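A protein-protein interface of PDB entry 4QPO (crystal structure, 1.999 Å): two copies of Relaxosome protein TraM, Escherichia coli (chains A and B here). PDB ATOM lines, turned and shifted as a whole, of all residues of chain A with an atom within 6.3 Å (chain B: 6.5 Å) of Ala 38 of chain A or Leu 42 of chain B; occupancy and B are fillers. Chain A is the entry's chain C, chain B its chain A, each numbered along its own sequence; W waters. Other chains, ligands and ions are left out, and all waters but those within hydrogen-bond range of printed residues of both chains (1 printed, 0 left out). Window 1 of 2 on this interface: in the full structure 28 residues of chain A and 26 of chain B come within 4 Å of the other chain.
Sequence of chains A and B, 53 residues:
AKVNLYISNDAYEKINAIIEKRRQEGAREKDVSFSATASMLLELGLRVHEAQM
Printed residues of chain A that touch a printed residue of chain B: Leu 5, Ile 7, Ala 11, Ile 15, Phe 34, Ser 35, Ala 38, Ser 39, Leu 41, Leu 42 and Gly 45.
Hydrophobic or aromatic side chains of chain A within 4 Å of the printed part of chain B: Leu 5, Ile 7, Ala 11, Ile 15, Phe 34, Ala 38, Leu 41 and Leu 42.
Along chain A the printed residues that touch a printed residue of chain B span positions 5 to 45.
Along chain B the printed residues that touch a printed residue of chain A span positions 3 to 46.
Among the printed residues, no Asp or Glu carboxylate lies within 4 Å of a Lys or Arg side-chain nitrogen of the other chain.
Water W1 bridges N of Asn 4 of chain B (3.2 Å) and OG of Ser 35 of chain A (3.2 Å).
Leu 5 of chain A touches Ala 38 of chain B, and with the chains exchanged Ala 38 of chain A touches Leu 5 of chain B.
Leu 5 of chain A touches Ser 39 of chain B, and with the chains exchanged Ser 39 of chain A touches Leu 5 of chain B.
Leu 41 of chain B touches its own counterpart, Leu 41 of chain A.
Leu 41 of chain A touches Leu 42 of chain B, and with the chains exchanged Leu 42 of chain A touches Leu 41 of chain B.
9 positions are printed for both chains.
Of the 24 pairs that touch across the chains among the printed residues, 13 have their exchanged pair printed and touching as well.
The backbone NH (N) of Val 3 of chain B lies within hydrogen-bond range of the backbone carbonyl oxygen (O) of Leu 5 of chain A.
O of Asn 4 of chain B lies within hydrogen-bond range of OG of Ser 35 of chain A, 3.0 Å away.
Ala 38 of chain B touches Leu 5 of chain A.
Ile 7 of chain A touches Val 3 of chain B.
CD2 of Leu 42 of chain B touches CG2 of Ile 7 of chain A, 3.7 Å away.
CD1 of Leu 46 of chain B touches CG1 of Ile 15 of chain A, at 3.9 Å.
Val 3 of chain B touches Phe 34 of chain A (CG1 to CE1, 3.4 Å).
Ala 38 of chain A touches Leu 5 of chain B.
Leu 42 of chain A touches Leu 41 of chain B (CD1 to CB, 3.4 Å).
CD1 of Leu 42 of chain A touches N of Leu 42 of chain B, 3.9 Å away.
Gly 45 of chain A touches Leu 44 of chain B (O to CD2, 3.6 Å).
Gly 45 of chain A touches Gly 45 of chain B (N to CA, 3.8 Å).
The backbone NH (N) of Ser 35 of chain A sits close to the side-chain hydroxyl (OG) of Ser 33 of chain A (3.5 Å).
The side-chain hydroxyl (OG) of Ser 39 of chain A lies within hydrogen-bond range of the backbone carbonyl oxygen (O) of Ser 35 of chain A (3.1 Å).
Ala 38 of chain A touches two residues of chain B.
Of chain A, only Ile 7 (3.7 Å), Ala 38 (3.3 Å), Leu 41 (3.5 Å) and Leu 42 (3.9 Å) come within 4 Å of Leu 42 of chain B.
Of the printed residues of chain A, Gly 45 of chain B touches Leu 41 (3.3 Å) and Gly 45 (3.8 Å).
Of the printed residues of chain A, Leu 5 of chain B touches Ser 35, Ala 38 and Ser 39.
The nearest residue of chain B that does not touch Ala 38 of chain A is Val 3 of chain B (5.3 Å).
The nearest printed residue of chain A that does not touch Leu 42 of chain B is Ile 15 of chain A (4.4 Å).
The nearest printed residue of chain A that does not touch Val 3 of chain B is Ala 38 of chain A (5.3 Å).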
ATOM      1  N   LEU A   5       6.822   5.714  22.457  1.00  0.00           N
ATOM      2  CA  LEU A   5       6.119   6.554  21.520  1.00  0.00           C
ATOM      3  C   LEU A   5       6.703   7.956  21.454  1.00  0.00           C
ATOM      4  O   LEU A   5       7.075   8.520  22.477  1.00  0.00           O
ATOM      5  CB  LEU A   5       4.650   6.614  21.931  1.00  0.00           C
ATOM      6  CG  LEU A   5       3.628   7.068  20.907  1.00  0.00           C
ATOM      7  CD1 LEU A   5       3.801   6.254  19.629  1.00  0.00           C
ATOM      8  CD2 LEU A   5       2.235   6.858  21.506  1.00  0.00           C
ATOM      9  N   ILE A   7       5.555  11.690  20.723  1.00  0.00           N
ATOM     10  CA  ILE A   7       4.348  12.495  20.625  1.00  0.00           C
ATOM     11  C   ILE A   7       4.726  13.942  20.269  1.00  0.00           C
ATOM     12  O   ILE A   7       5.908  14.304  20.297  1.00  0.00           O
ATOM     13  CB  ILE A   7       3.522  12.459  21.931  1.00  0.00           C
ATOM     14  CG1 ILE A   7       4.265  13.146  23.079  1.00  0.00           C
ATOM     15  CG2 ILE A   7       3.167  11.016  22.297  1.00  0.00           C
ATOM     16  CD1 ILE A   7       3.453  13.202  24.379  1.00  0.00           C
ATOM     17  N   ALA A  11       1.393  18.026  22.614  1.00  0.00           N
ATOM     18  CA  ALA A  11       0.775  17.012  23.491  1.00  0.00           C
ATOM     19  C   ALA A  11       1.597  16.858  24.769  1.00  0.00           C
ATOM     20  O   ALA A  11       1.064  16.749  25.871  1.00  0.00           O
ATOM     21  CB  ALA A  11       0.655  15.658  22.754  1.00  0.00           C
ATOM     22  N   ILE A  15       0.208  17.433  28.571  1.00  0.00           N
ATOM     23  CA  ILE A  15       0.290  16.441  29.640  1.00  0.00           C
ATOM     24  C   ILE A  15       1.074  16.993  30.836  1.00  0.00           C
ATOM     25  O   ILE A  15       0.664  16.797  31.969  1.00  0.00           O
ATOM     26  CB  ILE A  15       0.920  15.139  29.127  1.00  0.00           C
ATOM     27  CG1 ILE A  15       0.040  14.588  28.004  1.00  0.00           C
ATOM     28  CG2 ILE A  15       1.006  14.109  30.278  1.00  0.00           C
ATOM     29  CD1 ILE A  15       0.605  13.383  27.285  1.00  0.00           C
ATOM     30  N   SER A  33       2.397  11.190  37.822  1.00  0.00           N
ATOM     31  CA  SER A  33       3.330  10.516  36.912  1.00  0.00           C
ATOM     32  C   SER A  33       2.987  10.844  35.461  1.00  0.00           C
ATOM     33  O   SER A  33       1.837  10.699  35.023  1.00  0.00           O
ATOM     34  CB  SER A  33       3.317   9.000  37.147  1.00  0.00           C
ATOM     35  OG  SER A  33       3.804   8.279  36.032  1.00  0.00           O
ATOM     36  N   PHE A  34       3.988  11.288  34.710  1.00  0.00           N
ATOM     37  CA  PHE A  34       3.762  11.595  33.308  1.00  0.00           C
ATOM     38  C   PHE A  34       3.306  10.313  32.583  1.00  0.00           C
ATOM     39  O   PHE A  34       2.267  10.282  31.930  1.00  0.00           O
ATOM     40  CB  PHE A  34       5.021  12.149  32.650  1.00  0.00           C
ATOM     41  CG  PHE A  34       4.782  12.658  31.261  1.00  0.00           C
ATOM     42  CD1 PHE A  34       4.637  11.776  30.204  1.00  0.00           C
ATOM     43  CD2 PHE A  34       4.670  14.025  31.018  1.00  0.00           C
ATOM     44  CE1 PHE A  34       4.398  12.235  28.929  1.00  0.00           C
ATOM     45  CE2 PHE A  34       4.430  14.491  29.743  1.00  0.00           C
ATOM     46  CZ  PHE A  34       4.285  13.597  28.696  1.00  0.00           C
ATOM     47  N   SER A  35       4.099   9.276  32.742  1.00  0.00           N
ATOM     48  CA  SER A  35       3.849   7.971  32.136  1.00  0.00           C
ATOM     49  C   SER A  35       2.473   7.445  32.489  1.00  0.00           C
ATOM     50  O   SER A  35       1.754   6.954  31.611  1.00  0.00           O
ATOM     51  CB  SER A  35       4.920   6.955  32.569  1.00  0.00           C
ATOM     52  OG  SER A  35       6.160   7.305  31.997  1.00  0.00           O
ATOM     53  N   ALA A  36       2.100   7.537  33.762  1.00  0.00           N
ATOM     54  CA  ALA A  36       0.806   6.963  34.168  1.00  0.00           C
ATOM     55  C   ALA A  36      -0.335   7.778  33.575  1.00  0.00           C
ATOM     56  O   ALA A  36      -1.355   7.228  33.164  1.00  0.00           O
ATOM     57  CB  ALA A  36       0.677   6.902  35.678  1.00  0.00           C
ATOM     58  N   THR A  37      -0.166   9.097  33.528  1.00  0.00           N
ATOM     59  CA  THR A  37      -1.199   9.972  32.972  1.00  0.00           C
ATOM     60  C   THR A  37      -1.340   9.727  31.471  1.00  0.00           C
ATOM     61  O   THR A  37      -2.444   9.649  30.960  1.00  0.00           O
ATOM     62  CB  THR A  37      -0.867  11.457  33.257  1.00  0.00           C
ATOM     63  OG1 THR A  37      -0.763  11.609  34.676  1.00  0.00           O
ATOM     64  CG2 THR A  37      -1.958  12.401  32.757  1.00  0.00           C
ATOM     65  N   ALA A  38      -0.212   9.623  30.769  1.00  0.00           N
ATOM     66  CA  ALA A  38      -0.244   9.386  29.329  1.00  0.00           C
ATOM     67  C   ALA A  38      -0.923   8.057  29.016  1.00  0.00           C
ATOM     68  O   ALA A  38      -1.666   7.948  28.032  1.00  0.00           O
ATOM     69  CB  ALA A  38       1.151   9.406  28.757  1.00  0.00           C
ATOM     70  N   SER A  39      -0.694   7.050  29.862  1.00  0.00           N
ATOM     71  CA  SER A  39      -1.351   5.761  29.676  1.00  0.00           C
ATOM     72  C   SER A  39      -2.860   5.869  29.851  1.00  0.00           C
ATOM     73  O   SER A  39      -3.604   5.257  29.102  1.00  0.00           O
ATOM     74  CB  SER A  39      -0.809   4.723  30.641  1.00  0.00           C
ATOM     75  OG  SER A  39       0.515   4.389  30.292  1.00  0.00           O
ATOM     76  N   MET A  40      -3.300   6.631  30.849  1.00  0.00           N
ATOM     77  CA  MET A  40      -4.725   6.812  31.102  1.00  0.00           C
ATOM     78  C   MET A  40      -5.354   7.539  29.910  1.00  0.00           C
ATOM     79  O   MET A  40      -6.480   7.278  29.544  1.00  0.00           O
ATOM     80  CB  MET A  40      -4.943   7.594  32.412  1.00  0.00           C
ATOM     81  CG  MET A  40      -6.338   8.237  32.568  1.00  0.00           C
ATOM     82  SD  MET A  40      -6.376  10.024  32.262  1.00  0.00           S
ATOM     83  CE  MET A  40      -7.504  10.031  30.908  1.00  0.00           C
ATOM     84  N   LEU A  41      -4.626   8.482  29.320  1.00  0.00           N
ATOM     85  CA  LEU A  41      -5.160   9.229  28.180  1.00  0.00           C
ATOM     86  C   LEU A  41      -5.277   8.343  26.930  1.00  0.00           C
ATOM     87  O   LEU A  41      -6.236   8.460  26.155  1.00  0.00           O
ATOM     88  CB  LEU A  41      -4.277  10.453  27.883  1.00  0.00           C
ATOM     89  CG  LEU A  41      -4.330  11.557  28.955  1.00  0.00           C
ATOM     90  CD1 LEU A  41      -3.190  12.529  28.754  1.00  0.00           C
ATOM     91  CD2 LEU A  41      -5.669  12.287  28.943  1.00  0.00           C
ATOM     92  N   LEU A  42      -4.300   7.469  26.739  1.00  0.00           N
ATOM     93  CA  LEU A  42      -4.337   6.524  25.636  1.00  0.00           C
ATOM     94  C   LEU A  42      -5.545   5.583  25.778  1.00  0.00           C
ATOM     95  O   LEU A  42      -6.261   5.354  24.810  1.00  0.00           O
ATOM     96  CB  LEU A  42      -3.027   5.727  25.566  1.00  0.00           C
ATOM     97  CG  LEU A  42      -3.007   4.551  24.580  1.00  0.00           C
ATOM     98  CD1 LEU A  42      -3.382   5.006  23.208  1.00  0.00           C
ATOM     99  CD2 LEU A  42      -1.625   3.901  24.524  1.00  0.00           C
ATOM    100  N   GLU A  43      -5.766   5.051  26.980  1.00  0.00           N
ATOM    101  CA  GLU A  43      -6.960   4.241  27.261  1.00  0.00           C
ATOM    102  C   GLU A  43      -8.256   5.026  27.028  1.00  0.00           C
ATOM    103  O   GLU A  43      -9.239   4.466  26.531  1.00  0.00           O
ATOM    104  CB  GLU A  43      -6.950   3.720  28.701  1.00  0.00           C
ATOM    105  CG  GLU A  43      -5.815   2.759  29.048  1.00  0.00           C
ATOM    106  CD  GLU A  43      -6.261   1.302  29.124  1.00  0.00           C
ATOM    107  OE1 GLU A  43      -7.486   1.034  28.999  1.00  0.00           O
ATOM    108  OE2 GLU A  43      -5.380   0.417  29.300  1.00  0.00           O
ATOM    109  N   GLY A  45      -8.738   7.556  24.931  1.00  0.00           N
ATOM    110  CA  GLY A  45      -8.898   7.716  23.509  1.00  0.00           C
ATOM    111  C   GLY A  45      -9.374   6.417  22.889  1.00  0.00           C
ATOM    112  O   GLY A  45     -10.157   6.427  21.929  1.00  0.00           O
ATOM    113  N   VAL B   3       7.948   9.280  24.815  1.00  0.00           N
ATOM    114  CA  VAL B   3       7.309   8.832  26.066  1.00  0.00           C
ATOM    115  C   VAL B   3       7.337   7.314  26.200  1.00  0.00           C
ATOM    116  O   VAL B   3       7.317   6.581  25.212  1.00  0.00           O
ATOM    117  CB  VAL B   3       5.834   9.316  26.184  1.00  0.00           C
ATOM    118  CG1 VAL B   3       5.775  10.797  26.131  1.00  0.00           C
ATOM    119  CG2 VAL B   3       4.988   8.769  25.079  1.00  0.00           C
ATOM    120  N   ASN B   4       7.397   6.854  27.442  1.00  0.00           N
ATOM    121  CA  ASN B   4       7.395   5.434  27.751  1.00  0.00           C
ATOM    122  C   ASN B   4       6.133   5.098  28.491  1.00  0.00           C
ATOM    123  O   ASN B   4       5.897   5.621  29.571  1.00  0.00           O
ATOM    124  CB  ASN B   4       8.614   5.071  28.588  1.00  0.00           C
ATOM    125  CG  ASN B   4       9.887   5.579  27.977  1.00  0.00           C
ATOM    126  OD1 ASN B   4      10.558   6.448  28.537  1.00  0.00           O
ATOM    127  ND2 ASN B   4      10.215   5.067  26.794  1.00  0.00           N
ATOM    128  N   LEU B   5       5.300   4.256  27.895  1.00  0.00           N
ATOM    129  CA  LEU B   5       3.983   3.992  28.460  1.00  0.00           C
ATOM    130  C   LEU B   5       3.836   2.526  28.802  1.00  0.00           C
ATOM    131  O   LEU B   5       4.328   1.657  28.098  1.00  0.00           O
ATOM    132  CB  LEU B   5       2.857   4.397  27.495  1.00  0.00           C
ATOM    133  CG  LEU B   5       2.840   5.861  27.073  1.00  0.00           C
ATOM    134  CD1 LEU B   5       1.466   6.210  26.540  1.00  0.00           C
ATOM    135  CD2 LEU B   5       3.186   6.713  28.280  1.00  0.00           C
ATOM    136  N   THR B  37      -1.181   4.681  15.375  1.00  0.00           N
ATOM    137  CA  THR B  37      -2.502   4.498  15.949  1.00  0.00           C
ATOM    138  C   THR B  37      -2.503   4.828  17.440  1.00  0.00           C
ATOM    139  O   THR B  37      -3.379   5.549  17.918  1.00  0.00           O
ATOM    140  CB  THR B  37      -3.002   3.055  15.720  1.00  0.00           C
ATOM    141  OG1 THR B  37      -3.244   2.877  14.328  1.00  0.00           O
ATOM    142  CG2 THR B  37      -4.298   2.796  16.463  1.00  0.00           C
ATOM    143  N   ALA B  38      -1.517   4.305  18.158  1.00  0.00           N
ATOM    144  CA  ALA B  38      -1.349   4.582  19.574  1.00  0.00           C
ATOM    145  C   ALA B  38      -1.225   6.078  19.834  1.00  0.00           C
ATOM    146  O   ALA B  38      -1.830   6.614  20.749  1.00  0.00           O
ATOM    147  CB  ALA B  38      -0.116   3.852  20.111  1.00  0.00           C
ATOM    148  N   SER B  39      -0.428   6.740  19.016  1.00  0.00           N
ATOM    149  CA  SER B  39      -0.183   8.160  19.165  1.00  0.00           C
ATOM    150  C   SER B  39      -1.462   8.935  18.876  1.00  0.00           C
ATOM    151  O   SER B  39      -1.789   9.925  19.545  1.00  0.00           O
ATOM    152  CB  SER B  39       0.960   8.568  18.231  1.00  0.00           C
ATOM    153  OG  SER B  39       1.064   9.970  18.127  1.00  0.00           O
ATOM    154  N   MET B  40      -2.209   8.450  17.894  1.00  0.00           N
ATOM    155  CA  MET B  40      -3.468   9.066  17.516  1.00  0.00           C
ATOM    156  C   MET B  40      -4.472   8.936  18.643  1.00  0.00           C
ATOM    157  O   MET B  40      -5.257   9.843  18.890  1.00  0.00           O
ATOM    158  CB  MET B  40      -4.024   8.429  16.234  1.00  0.00           C
ATOM    159  CG  MET B  40      -5.202   9.180  15.622  1.00  0.00           C
ATOM    160  SD  MET B  40      -6.628   8.121  15.300  1.00  0.00           S
ATOM    161  CE  MET B  40      -7.162   7.821  16.968  1.00  0.00           C
ATOM    162  N   LEU B  41      -4.447   7.802  19.326  1.00  0.00           N
ATOM    163  CA  LEU B  41      -5.395   7.563  20.397  1.00  0.00           C
ATOM    164  C   LEU B  41      -5.064   8.387  21.639  1.00  0.00           C
ATOM    165  O   LEU B  41      -5.972   8.800  22.378  1.00  0.00           O
ATOM    166  CB  LEU B  41      -5.445   6.080  20.736  1.00  0.00           C
ATOM    167  CG  LEU B  41      -6.161   5.183  19.736  1.00  0.00           C
ATOM    168  CD1 LEU B  41      -5.896   3.758  20.110  1.00  0.00           C
ATOM    169  CD2 LEU B  41      -7.666   5.471  19.727  1.00  0.00           C
ATOM    170  N   LEU B  42      -3.774   8.651  21.839  1.00  0.00           N
ATOM    171  CA  LEU B  42      -3.304   9.430  22.981  1.00  0.00           C
ATOM    172  C   LEU B  42      -3.669  10.904  22.812  1.00  0.00           C
ATOM    173  O   LEU B  42      -4.067  11.579  23.772  1.00  0.00           O
ATOM    174  CB  LEU B  42      -1.783   9.269  23.153  1.00  0.00           C
ATOM    175  CG  LEU B  42      -1.038  10.150  24.169  1.00  0.00           C
ATOM    176  CD1 LEU B  42      -1.659  10.100  25.533  1.00  0.00           C
ATOM    177  CD2 LEU B  42       0.378   9.690  24.258  1.00  0.00           C
ATOM    178  N   GLU B  43      -3.540  11.406  21.588  1.00  0.00           N
ATOM    179  CA  GLU B  43      -3.877  12.797  21.331  1.00  0.00           C
ATOM    180  C   GLU B  43      -5.399  12.998  21.333  1.00  0.00           C
ATOM    181  O   GLU B  43      -5.855  14.061  21.723  1.00  0.00           O
ATOM    182  CB  GLU B  43      -3.251  13.266  20.018  1.00  0.00           C
ATOM    183  CG  GLU B  43      -1.723  13.295  20.135  1.00  0.00           C
ATOM    184  CD  GLU B  43      -1.038  13.923  18.964  1.00  0.00           C
ATOM    185  OE1 GLU B  43      -1.595  13.848  17.843  1.00  0.00           O
ATOM    186  OE2 GLU B  43       0.070  14.482  19.161  1.00  0.00           O
ATOM    187  N   LEU B  44      -6.152  11.995  20.886  1.00  0.00           N
ATOM    188  CA  LEU B  44      -7.621  11.965  21.028  1.00  0.00           C
ATOM    189  C   LEU B  44      -8.020  12.032  22.504  1.00  0.00           C
ATOM    190  O   LEU B  44      -8.882  12.818  22.910  1.00  0.00           O
ATOM    191  CB  LEU B  44      -8.206  10.695  20.404  1.00  0.00           C
ATOM    192  CG  LEU B  44      -9.738  10.476  20.546  1.00  0.00           C
ATOM    193  CD1 LEU B  44     -10.520  11.707  20.139  1.00  0.00           C
ATOM    194  CD2 LEU B  44     -10.219   9.301  19.731  1.00  0.00           C
ATOM    195  N   GLY B  45      -7.405  11.165  23.295  1.00  0.00           N
ATOM    196  CA  GLY B  45      -7.618  11.142  24.728  1.00  0.00           C
ATOM    197  C   GLY B  45      -7.330  12.482  25.374  1.00  0.00           C
ATOM    198  O   GLY B  45      -8.051  12.894  26.260  1.00  0.00           O
ATOM    199  N   LEU B  46      -6.276  13.161  24.921  1.00  0.00           N
ATOM    200  CA  LEU B  46      -5.998  14.515  25.342  1.00  0.00           C
ATOM    201  C   LEU B  46      -7.102  15.500  24.966  1.00  0.00           C
ATOM    202  O   LEU B  46      -7.506  16.316  25.786  1.00  0.00           O
ATOM    203  CB  LEU B  46      -4.662  14.957  24.734  1.00  0.00           C
ATOM    204  CG  LEU B  46      -3.747  15.875  25.491  1.00  0.00           C
ATOM    205  CD1 LEU B  46      -3.562  15.494  26.941  1.00  0.00           C
ATOM    206  CD2 LEU B  46      -2.421  15.892  24.763  1.00  0.00           C
ATOM    207  N   ARG B  47      -7.609  15.427  23.733  1.00  0.00           N
ATOM    208  CA  ARG B  47      -8.689  16.320  23.342  1.00  0.00           C
ATOM    209  C   ARG B  47      -9.957  15.968  24.115  1.00  0.00           C
ATOM    210  O   ARG B  47     -10.737  16.844  24.478  1.00  0.00           O
ATOM    211  CB  ARG B  47      -8.928  16.254  21.835  1.00  0.00           C
ATOM    212  CG  ARG B  47      -7.721  16.764  21.025  1.00  0.00           C
ATOM    213  CD  ARG B  47      -8.083  16.956  19.565  1.00  0.00           C
ATOM    214  NE  ARG B  47      -8.689  15.768  18.976  1.00  0.00           N
ATOM    215  CZ  ARG B  47      -8.021  14.757  18.412  1.00  0.00           C
ATOM    216  NH1 ARG B  47      -6.690  14.754  18.365  1.00  0.00           N
ATOM    217  NH2 ARG B  47      -8.691  13.740  17.888  1.00  0.00           N
HETATM  218  O   HOH W   1       7.808   8.916  29.788  1.00  0.00           O
